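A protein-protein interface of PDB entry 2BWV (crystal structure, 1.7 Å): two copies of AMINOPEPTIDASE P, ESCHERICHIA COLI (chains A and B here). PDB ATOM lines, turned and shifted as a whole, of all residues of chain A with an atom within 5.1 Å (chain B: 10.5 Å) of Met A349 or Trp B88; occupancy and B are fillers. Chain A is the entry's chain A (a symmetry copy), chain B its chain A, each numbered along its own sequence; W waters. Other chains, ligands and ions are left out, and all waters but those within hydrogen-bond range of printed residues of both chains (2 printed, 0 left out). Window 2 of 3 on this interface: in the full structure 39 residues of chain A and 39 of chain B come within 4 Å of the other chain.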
ATOM      1  N   ILE A 241      -1.010  13.318  21.748  1.00  0.00           N
ATOM      2  CA  ILE A 241      -1.085  14.711  22.187  1.00  0.00           C
ATOM      3  C   ILE A 241      -1.875  14.767  23.496  1.00  0.00           C
ATOM      4  O   ILE A 241      -3.059  14.387  23.541  1.00  0.00           O
ATOM      5  CB  ILE A 241      -1.764  15.580  21.105  1.00  0.00           C
ATOM      6  CG1 ILE A 241      -0.940  15.572  19.825  1.00  0.00           C
ATOM      7  CG2 ILE A 241      -1.969  17.012  21.610  1.00  0.00           C
ATOM      8  CD1 ILE A 241      -1.679  16.155  18.617  1.00  0.00           C
ATOM      9  N   LEU A 242      -1.230  15.222  24.573  1.00  0.00           N
ATOM     10  CA  LEU A 242      -1.777  15.057  25.922  1.00  0.00           C
ATOM     11  C   LEU A 242      -3.155  15.712  26.220  1.00  0.00           C
ATOM     12  O   LEU A 242      -4.018  15.094  26.870  1.00  0.00           O
ATOM     13  CB  LEU A 242      -0.746  15.513  26.972  1.00  0.00           C
ATOM     14  CG  LEU A 242       0.558  14.687  26.996  1.00  0.00           C
ATOM     15  CD1 LEU A 242       1.466  15.152  28.134  1.00  0.00           C
ATOM     16  CD2 LEU A 242       0.282  13.176  27.093  1.00  0.00           C
ATOM     17  N   HIS A 243      -3.309  16.957  25.812  1.00  0.00           N
ATOM     18  CA  HIS A 243      -4.572  17.706  25.980  1.00  0.00           C
ATOM     19  C   HIS A 243      -5.185  17.989  24.597  1.00  0.00           C
ATOM     20  O   HIS A 243      -5.631  19.105  24.313  1.00  0.00           O
ATOM     21  CB  HIS A 243      -4.332  19.023  26.736  1.00  0.00           C
ATOM     22  CG  HIS A 243      -3.697  18.849  28.087  1.00  0.00           C
ATOM     23  ND1 HIS A 243      -2.333  18.736  28.261  1.00  0.00           N
ATOM     24  CD2 HIS A 243      -4.239  18.793  29.327  1.00  0.00           C
ATOM     25  CE1 HIS A 243      -2.064  18.597  29.548  1.00  0.00           C
ATOM     26  NE2 HIS A 243      -3.203  18.630  30.216  1.00  0.00           N
ATOM     27  N   TYR A 244      -5.191  16.970  23.739  1.00  0.00           N
ATOM     28  CA  TYR A 244      -5.839  17.048  22.427  1.00  0.00           C
ATOM     29  C   TYR A 244      -7.339  17.280  22.614  1.00  0.00           C
ATOM     30  O   TYR A 244      -8.039  16.390  23.088  1.00  0.00           O
ATOM     31  CB  TYR A 244      -5.617  15.732  21.667  1.00  0.00           C
ATOM     32  CG  TYR A 244      -6.353  15.661  20.351  1.00  0.00           C
ATOM     33  CD1 TYR A 244      -5.870  16.324  19.227  1.00  0.00           C
ATOM     34  CD2 TYR A 244      -7.559  14.948  20.236  1.00  0.00           C
ATOM     35  CE1 TYR A 244      -6.548  16.285  18.013  1.00  0.00           C
ATOM     36  CE2 TYR A 244      -8.247  14.899  19.017  1.00  0.00           C
ATOM     37  CZ  TYR A 244      -7.736  15.556  17.909  1.00  0.00           C
ATOM     38  OH  TYR A 244      -8.423  15.510  16.707  1.00  0.00           O
ATOM     39  N   ARG A 345      11.277   8.936  29.961  1.00  0.00           N
ATOM     40  CA  ARG A 345      10.668  10.269  29.794  1.00  0.00           C
ATOM     41  C   ARG A 345      10.176  10.660  28.390  1.00  0.00           C
ATOM     42  O   ARG A 345       9.210  11.421  28.280  1.00  0.00           O
ATOM     43  CB  ARG A 345      11.584  11.363  30.349  1.00  0.00           C
ATOM     44  CG  ARG A 345      11.618  11.391  31.871  1.00  0.00           C
ATOM     45  CD  ARG A 345      12.407  12.619  32.335  1.00  0.00           C
ATOM     46  NE  ARG A 345      12.438  12.788  33.790  1.00  0.00           N
ATOM     47  CZ  ARG A 345      13.338  13.517  34.453  1.00  0.00           C
ATOM     48  NH1 ARG A 345      14.317  14.151  33.811  1.00  0.00           N
ATOM     49  NH2 ARG A 345      13.263  13.604  35.776  1.00  0.00           N
ATOM     50  N   PRO A 346      10.825  10.158  27.325  1.00  0.00           N
ATOM     51  CA  PRO A 346      10.270  10.400  25.985  1.00  0.00           C
ATOM     52  C   PRO A 346       8.886   9.783  25.770  1.00  0.00           C
ATOM     53  O   PRO A 346       8.159  10.226  24.886  1.00  0.00           O
ATOM     54  CB  PRO A 346      11.292   9.751  25.046  1.00  0.00           C
ATOM     55  CG  PRO A 346      12.563   9.671  25.858  1.00  0.00           C
ATOM     56  CD  PRO A 346      12.100   9.415  27.258  1.00  0.00           C
ATOM     57  N   PHE A 347       8.531   8.782  26.579  1.00  0.00           N
ATOM     58  CA  PHE A 347       7.289   8.028  26.409  1.00  0.00           C
ATOM     59  C   PHE A 347       6.282   8.263  27.530  1.00  0.00           C
ATOM     60  O   PHE A 347       5.086   8.116  27.307  1.00  0.00           O
ATOM     61  CB  PHE A 347       7.619   6.530  26.297  1.00  0.00           C
ATOM     62  CG  PHE A 347       8.672   6.236  25.269  1.00  0.00           C
ATOM     63  CD1 PHE A 347       8.406   6.454  23.914  1.00  0.00           C
ATOM     64  CD2 PHE A 347       9.937   5.809  25.640  1.00  0.00           C
ATOM     65  CE1 PHE A 347       9.374   6.213  22.953  1.00  0.00           C
ATOM     66  CE2 PHE A 347      10.916   5.562  24.680  1.00  0.00           C
ATOM     67  CZ  PHE A 347      10.637   5.767  23.339  1.00  0.00           C
ATOM     68  N   PHE A 348       6.772   8.583  28.734  1.00  0.00           N
ATOM     69  CA  PHE A 348       5.918   8.945  29.868  1.00  0.00           C
ATOM     70  C   PHE A 348       6.469  10.254  30.444  1.00  0.00           C
ATOM     71  O   PHE A 348       7.426  10.249  31.233  1.00  0.00           O
ATOM     72  CB  PHE A 348       5.886   7.833  30.916  1.00  0.00           C
ATOM     73  CG  PHE A 348       5.135   8.192  32.179  1.00  0.00           C
ATOM     74  CD1 PHE A 348       3.835   8.692  32.124  1.00  0.00           C
ATOM     75  CD2 PHE A 348       5.719   7.985  33.434  1.00  0.00           C
ATOM     76  CE1 PHE A 348       3.140   8.993  33.285  1.00  0.00           C
ATOM     77  CE2 PHE A 348       5.037   8.293  34.598  1.00  0.00           C
ATOM     78  CZ  PHE A 348       3.747   8.786  34.537  1.00  0.00           C
ATOM     79  N   MET A 349       5.889  11.366  30.000  1.00  0.00           N
ATOM     80  CA  MET A 349       6.499  12.689  30.222  1.00  0.00           C
ATOM     81  C   MET A 349       5.748  13.575  31.205  1.00  0.00           C
ATOM     82  O   MET A 349       6.115  14.753  31.386  1.00  0.00           O
ATOM     83  CB  MET A 349       6.662  13.429  28.884  1.00  0.00           C
ATOM     84  CG  MET A 349       5.365  13.844  28.193  1.00  0.00           C
ATOM     85  SD  MET A 349       4.437  12.464  27.495  1.00  0.00           S
ATOM     86  CE  MET A 349       5.599  11.776  26.323  1.00  0.00           C
ATOM     87  N   HIS A 350       4.692  13.042  31.819  1.00  0.00           N
ATOM     88  CA  HIS A 350       3.880  13.798  32.750  1.00  0.00           C
ATOM     89  C   HIS A 350       3.828  13.108  34.122  1.00  0.00           C
ATOM     90  O   HIS A 350       4.423  12.032  34.319  1.00  0.00           O
ATOM     91  CB  HIS A 350       2.482  14.058  32.171  1.00  0.00           C
ATOM     92  CG  HIS A 350       1.683  12.819  31.891  1.00  0.00           C
ATOM     93  ND1 HIS A 350       1.031  12.117  32.886  1.00  0.00           N
ATOM     94  CD2 HIS A 350       1.386  12.188  30.726  1.00  0.00           C
ATOM     95  CE1 HIS A 350       0.389  11.092  32.345  1.00  0.00           C
ATOM     96  NE2 HIS A 350       0.584  11.115  31.039  1.00  0.00           N
ATOM     97  N   GLY A 351       3.180  13.768  35.076  1.00  0.00           N
ATOM     98  CA  GLY A 351       3.070  13.241  36.442  1.00  0.00           C
ATOM     99  C   GLY A 351       2.080  12.091  36.528  1.00  0.00           C
ATOM    100  O   GLY A 351       1.144  11.989  35.732  1.00  0.00           O
ATOM    101  N   TYR A 387       3.211   7.085  25.397  1.00  0.00           N
ATOM    102  CA  TYR A 387       2.908   7.792  24.150  1.00  0.00           C
ATOM    103  C   TYR A 387       4.110   7.606  23.252  1.00  0.00           C
ATOM    104  O   TYR A 387       5.194   8.115  23.548  1.00  0.00           O
ATOM    105  CB  TYR A 387       2.619   9.276  24.409  1.00  0.00           C
ATOM    106  CG  TYR A 387       1.740   9.483  25.625  1.00  0.00           C
ATOM    107  CD1 TYR A 387       2.302   9.678  26.901  1.00  0.00           C
ATOM    108  CD2 TYR A 387       0.352   9.403  25.530  1.00  0.00           C
ATOM    109  CE1 TYR A 387       1.502   9.838  28.028  1.00  0.00           C
ATOM    110  CE2 TYR A 387      -0.458   9.561  26.648  1.00  0.00           C
ATOM    111  CZ  TYR A 387       0.115   9.768  27.905  1.00  0.00           C
ATOM    112  OH  TYR A 387      -0.687   9.918  29.020  1.00  0.00           O
ATOM    113  N   ARG B  79       1.292  31.611  16.424  1.00  0.00           N
ATOM    114  CA  ARG B  79       2.199  30.834  17.255  1.00  0.00           C
ATOM    115  C   ARG B  79       3.133  29.954  16.443  1.00  0.00           C
ATOM    116  O   ARG B  79       2.721  29.307  15.477  1.00  0.00           O
ATOM    117  CB  ARG B  79       1.424  29.955  18.219  1.00  0.00           C
ATOM    118  CG  ARG B  79       0.716  30.739  19.283  1.00  0.00           C
ATOM    119  CD  ARG B  79      -0.326  29.848  19.945  1.00  0.00           C
ATOM    120  NE  ARG B  79      -0.613  30.336  21.280  1.00  0.00           N
ATOM    121  CZ  ARG B  79      -1.425  29.732  22.141  1.00  0.00           C
ATOM    122  NH1 ARG B  79      -2.046  28.610  21.799  1.00  0.00           N
ATOM    123  NH2 ARG B  79      -1.613  30.264  23.344  1.00  0.00           N
ATOM    124  N   ASP B  82       6.284  24.263  17.889  1.00  0.00           N
ATOM    125  CA  ASP B  82       7.086  23.931  19.056  1.00  0.00           C
ATOM    126  C   ASP B  82       6.709  22.527  19.498  1.00  0.00           C
ATOM    127  O   ASP B  82       5.601  22.300  19.990  1.00  0.00           O
ATOM    128  CB  ASP B  82       6.831  24.918  20.194  1.00  0.00           C
ATOM    129  CG  ASP B  82       7.696  24.630  21.409  1.00  0.00           C
ATOM    130  OD1 ASP B  82       7.227  23.911  22.320  1.00  0.00           O
ATOM    131  OD2 ASP B  82       8.864  25.083  21.424  1.00  0.00           O
ATOM    132  N   LEU B  83       7.639  21.598  19.339  1.00  0.00           N
ATOM    133  CA  LEU B  83       7.363  20.186  19.592  1.00  0.00           C
ATOM    134  C   LEU B  83       6.745  19.957  20.972  1.00  0.00           C
ATOM    135  O   LEU B  83       5.695  19.311  21.083  1.00  0.00           O
ATOM    136  CB  LEU B  83       8.637  19.354  19.439  1.00  0.00           C
ATOM    137  CG  LEU B  83       8.412  17.839  19.489  1.00  0.00           C
ATOM    138  CD1 LEU B  83       7.318  17.414  18.494  1.00  0.00           C
ATOM    139  CD2 LEU B  83       9.717  17.082  19.236  1.00  0.00           C
ATOM    140  N   THR B  84       7.378  20.501  22.010  1.00  0.00           N
ATOM    141  CA  THR B  84       6.927  20.260  23.390  1.00  0.00           C
ATOM    142  C   THR B  84       5.540  20.856  23.676  1.00  0.00           C
ATOM    143  O   THR B  84       4.674  20.177  24.233  1.00  0.00           O
ATOM    144  CB  THR B  84       7.962  20.778  24.422  1.00  0.00           C
ATOM    145  OG1 THR B  84       9.179  20.045  24.269  1.00  0.00           O
ATOM    146  CG2 THR B  84       7.455  20.600  25.863  1.00  0.00           C
ATOM    147  N   ALA B  85       5.330  22.116  23.296  1.00  0.00           N
ATOM    148  CA  ALA B  85       4.028  22.763  23.505  1.00  0.00           C
ATOM    149  C   ALA B  85       2.923  22.004  22.763  1.00  0.00           C
ATOM    150  O   ALA B  85       1.788  21.876  23.256  1.00  0.00           O
ATOM    151  CB  ALA B  85       4.069  24.234  23.054  1.00  0.00           C
ATOM    152  N   GLU B  86       3.273  21.484  21.586  1.00  0.00           N
ATOM    153  CA  GLU B  86       2.313  20.747  20.780  1.00  0.00           C
ATOM    154  C   GLU B  86       1.991  19.361  21.341  1.00  0.00           C
ATOM    155  O   GLU B  86       0.824  19.005  21.373  1.00  0.00           O
ATOM    156  CB  GLU B  86       2.749  20.693  19.315  1.00  0.00           C
ATOM    157  CG  GLU B  86       2.646  22.076  18.668  1.00  0.00           C
ATOM    158  CD  GLU B  86       3.011  22.057  17.218  1.00  0.00           C
ATOM    159  OE1 GLU B  86       2.329  21.337  16.450  1.00  0.00           O
ATOM    160  OE2 GLU B  86       3.984  22.759  16.859  1.00  0.00           O
ATOM    161  N   ILE B  87       2.996  18.610  21.788  1.00  0.00           N
ATOM    162  CA  ILE B  87       2.752  17.338  22.513  1.00  0.00           C
ATOM    163  C   ILE B  87       1.798  17.571  23.684  1.00  0.00           C
ATOM    164  O   ILE B  87       0.896  16.774  23.946  1.00  0.00           O
ATOM    165  CB  ILE B  87       4.056  16.709  23.070  1.00  0.00           C
ATOM    166  CG1 ILE B  87       4.913  16.153  21.930  1.00  0.00           C
ATOM    167  CG2 ILE B  87       3.740  15.606  24.088  1.00  0.00           C
ATOM    168  CD1 ILE B  87       6.355  15.866  22.333  1.00  0.00           C
ATOM    169  N   TRP B  88       2.009  18.657  24.405  1.00  0.00           N
ATOM    170  CA  TRP B  88       1.172  18.937  25.564  1.00  0.00           C
ATOM    171  C   TRP B  88      -0.239  19.428  25.207  1.00  0.00           C
ATOM    172  O   TRP B  88      -1.237  18.881  25.700  1.00  0.00           O
ATOM    173  CB  TRP B  88       1.907  19.893  26.514  1.00  0.00           C
ATOM    174  CG  TRP B  88       2.896  19.136  27.352  1.00  0.00           C
ATOM    175  CD1 TRP B  88       4.132  18.705  26.974  1.00  0.00           C
ATOM    176  CD2 TRP B  88       2.697  18.661  28.692  1.00  0.00           C
ATOM    177  NE1 TRP B  88       4.727  18.005  28.006  1.00  0.00           N
ATOM    178  CE2 TRP B  88       3.863  17.966  29.067  1.00  0.00           C
ATOM    179  CE3 TRP B  88       1.647  18.764  29.611  1.00  0.00           C
ATOM    180  CZ2 TRP B  88       4.013  17.378  30.328  1.00  0.00           C
ATOM    181  CZ3 TRP B  88       1.798  18.181  30.865  1.00  0.00           C
ATOM    182  CH2 TRP B  88       2.972  17.502  31.209  1.00  0.00           C
ATOM    183  N   PHE B  89      -0.328  20.418  24.321  1.00  0.00           N
ATOM    184  CA  PHE B  89      -1.548  21.229  24.202  1.00  0.00           C
ATOM    185  C   PHE B  89      -2.239  21.220  22.841  1.00  0.00           C
ATOM    186  O   PHE B  89      -3.380  21.687  22.721  1.00  0.00           O
ATOM    187  CB  PHE B  89      -1.237  22.665  24.633  1.00  0.00           C
ATOM    188  CG  PHE B  89      -0.691  22.757  26.040  1.00  0.00           C
ATOM    189  CD1 PHE B  89      -1.450  22.303  27.123  1.00  0.00           C
ATOM    190  CD2 PHE B  89       0.575  23.271  26.285  1.00  0.00           C
ATOM    191  CE1 PHE B  89      -0.957  22.368  28.419  1.00  0.00           C
ATOM    192  CE2 PHE B  89       1.074  23.340  27.582  1.00  0.00           C
ATOM    193  CZ  PHE B  89       0.306  22.890  28.648  1.00  0.00           C
ATOM    194  N   GLY B  90      -1.565  20.688  21.827  1.00  0.00           N
ATOM    195  CA  GLY B  90      -2.180  20.548  20.531  1.00  0.00           C
ATOM    196  C   GLY B  90      -1.351  21.129  19.424  1.00  0.00           C
ATOM    197  O   GLY B  90      -0.428  21.924  19.649  1.00  0.00           O
ATOM    198  N   ARG B  91      -1.718  20.742  18.216  1.00  0.00           N
ATOM    199  CA  ARG B  91      -0.950  21.109  17.057  1.00  0.00           C
ATOM    200  C   ARG B  91      -1.147  22.590  16.792  1.00  0.00           C
ATOM    201  O   ARG B  91      -2.182  23.179  17.141  1.00  0.00           O
ATOM    202  CB  ARG B  91      -1.363  20.285  15.846  1.00  0.00           C
ATOM    203  CG  ARG B  91      -1.153  18.792  16.016  1.00  0.00           C
ATOM    204  CD  ARG B  91      -1.339  18.080  14.695  1.00  0.00           C
ATOM    205  NE  ARG B  91      -1.181  16.642  14.855  1.00  0.00           N
ATOM    206  CZ  ARG B  91      -2.135  15.813  15.288  1.00  0.00           C
ATOM    207  NH1 ARG B  91      -3.344  16.274  15.599  1.00  0.00           N
ATOM    208  NH2 ARG B  91      -1.869  14.520  15.398  1.00  0.00           N
ATOM    209  N   ARG B  92      -0.118  23.183  16.208  1.00  0.00           N
ATOM    210  CA  ARG B  92      -0.131  24.582  15.817  1.00  0.00           C
ATOM    211  C   ARG B  92       0.161  24.631  14.344  1.00  0.00           C
ATOM    212  O   ARG B  92       0.949  23.824  13.817  1.00  0.00           O
ATOM    213  CB  ARG B  92       0.964  25.344  16.542  1.00  0.00           C
ATOM    214  CG  ARG B  92       0.769  25.422  18.019  1.00  0.00           C
ATOM    215  CD  ARG B  92       2.037  25.921  18.655  1.00  0.00           C
ATOM    216  NE  ARG B  92       1.849  26.251  20.060  1.00  0.00           N
ATOM    217  CZ  ARG B  92       2.651  27.047  20.764  1.00  0.00           C
ATOM    218  NH1 ARG B  92       3.714  27.632  20.207  1.00  0.00           N
ATOM    219  NH2 ARG B  92       2.373  27.274  22.040  1.00  0.00           N
HETATM  220  O   HOH W   1      -4.939  21.875  25.535  1.00  0.00           O
HETATM  221  O   HOH W   2      -6.009  20.784  21.724  1.00  0.00           O
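The backbone carbonyl oxygen (O) of Ile B87 lies within hydrogen-bond range of the backbone NH (N) of Leu A242.
The backbone carbonyl oxygen of Trp B88 sits at hydrogen-bond distance from a ring nitrogen (ND1) of His A243 (2.8 Å).
Of the 12 printed residues of chain B, 6 touch a printed residue of chain A.
Printed residues of chain B that touch a printed residue of chain A: Glu B86, Ile B87, Trp B88, Phe B89, Gly B90 and Arg B91.
Of the 12 printed residues of chain A, 5 touch a printed residue of chain B.
Among the printed residues, no Asp or Glu carboxylate lies within 4 Å of a Lys or Arg side-chain nitrogen of the other chain.
Water W2 bridges the backbone carbonyl oxygen (O) of Phe B89 (3.0 Å) and the backbone carbonyl oxygen (O) of His A243 (3.1 Å).
Water W1 lies within hydrogen-bond range of O of His A243 and O of Phe B89.
Met A349 touches just one residue of chain B: Trp B88.
Trp B88 touches four residues of chain A.
Of chain B, only Trp B88 and Phe B89 come within 4 Å of His A243.
No residue of chain B comes within 4 Å of Phe A348.
Of the printed residues of chain A, Gly B90 touches Ile A241 (3.7 Å).
Of the printed residues of chain A, Glu B86 touches Ile A241 (3.4 Å).
Printed residues of chain B within 4 Å of Ile A241: Glu B86 (3.4 Å), Ile B87 (3.4 Å), Gly B90 (3.7 Å) and Arg B91 (3.4 Å).
Arg B79 touches none of the printed residues of chain A.
Leu B83 touches none of the printed residues of chain A.
The nearest residue of chain B that does not touch Met A349 is Ile B87 (4.7 Å).
The nearest residue of chain A that does not touch Trp B88 is Ile A241 (4.6 Å).
The nearest printed residue of chain B that does not touch Ile A241 is Phe B89 (4.4 Å).
The backbone NH (N) of Asp B82 lies within hydrogen-bond range of the side-chain carboxylate (OE2) of Glu B86 (2.9 Å).
The side-chain carboxylate (OE1) of Glu B86 lies within hydrogen-bond range of the backbone NH (N) of Arg B92 (3.1 Å).
NE2 of His A350 is in hydrogen-bond range of OH of Tyr A387 (2.7 Å).
Among the printed residues, merely in contact across the chains: Ile A241 with Ile B87, Ile A241 with Arg B91, Ile A241 with Glu B86, Met A349 with Trp B88, His A350 with Trp B88, Leu A242 with Trp B88, Ile A241 with Gly B90 and His A243 with Phe B89.
No position is printed for both chains.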
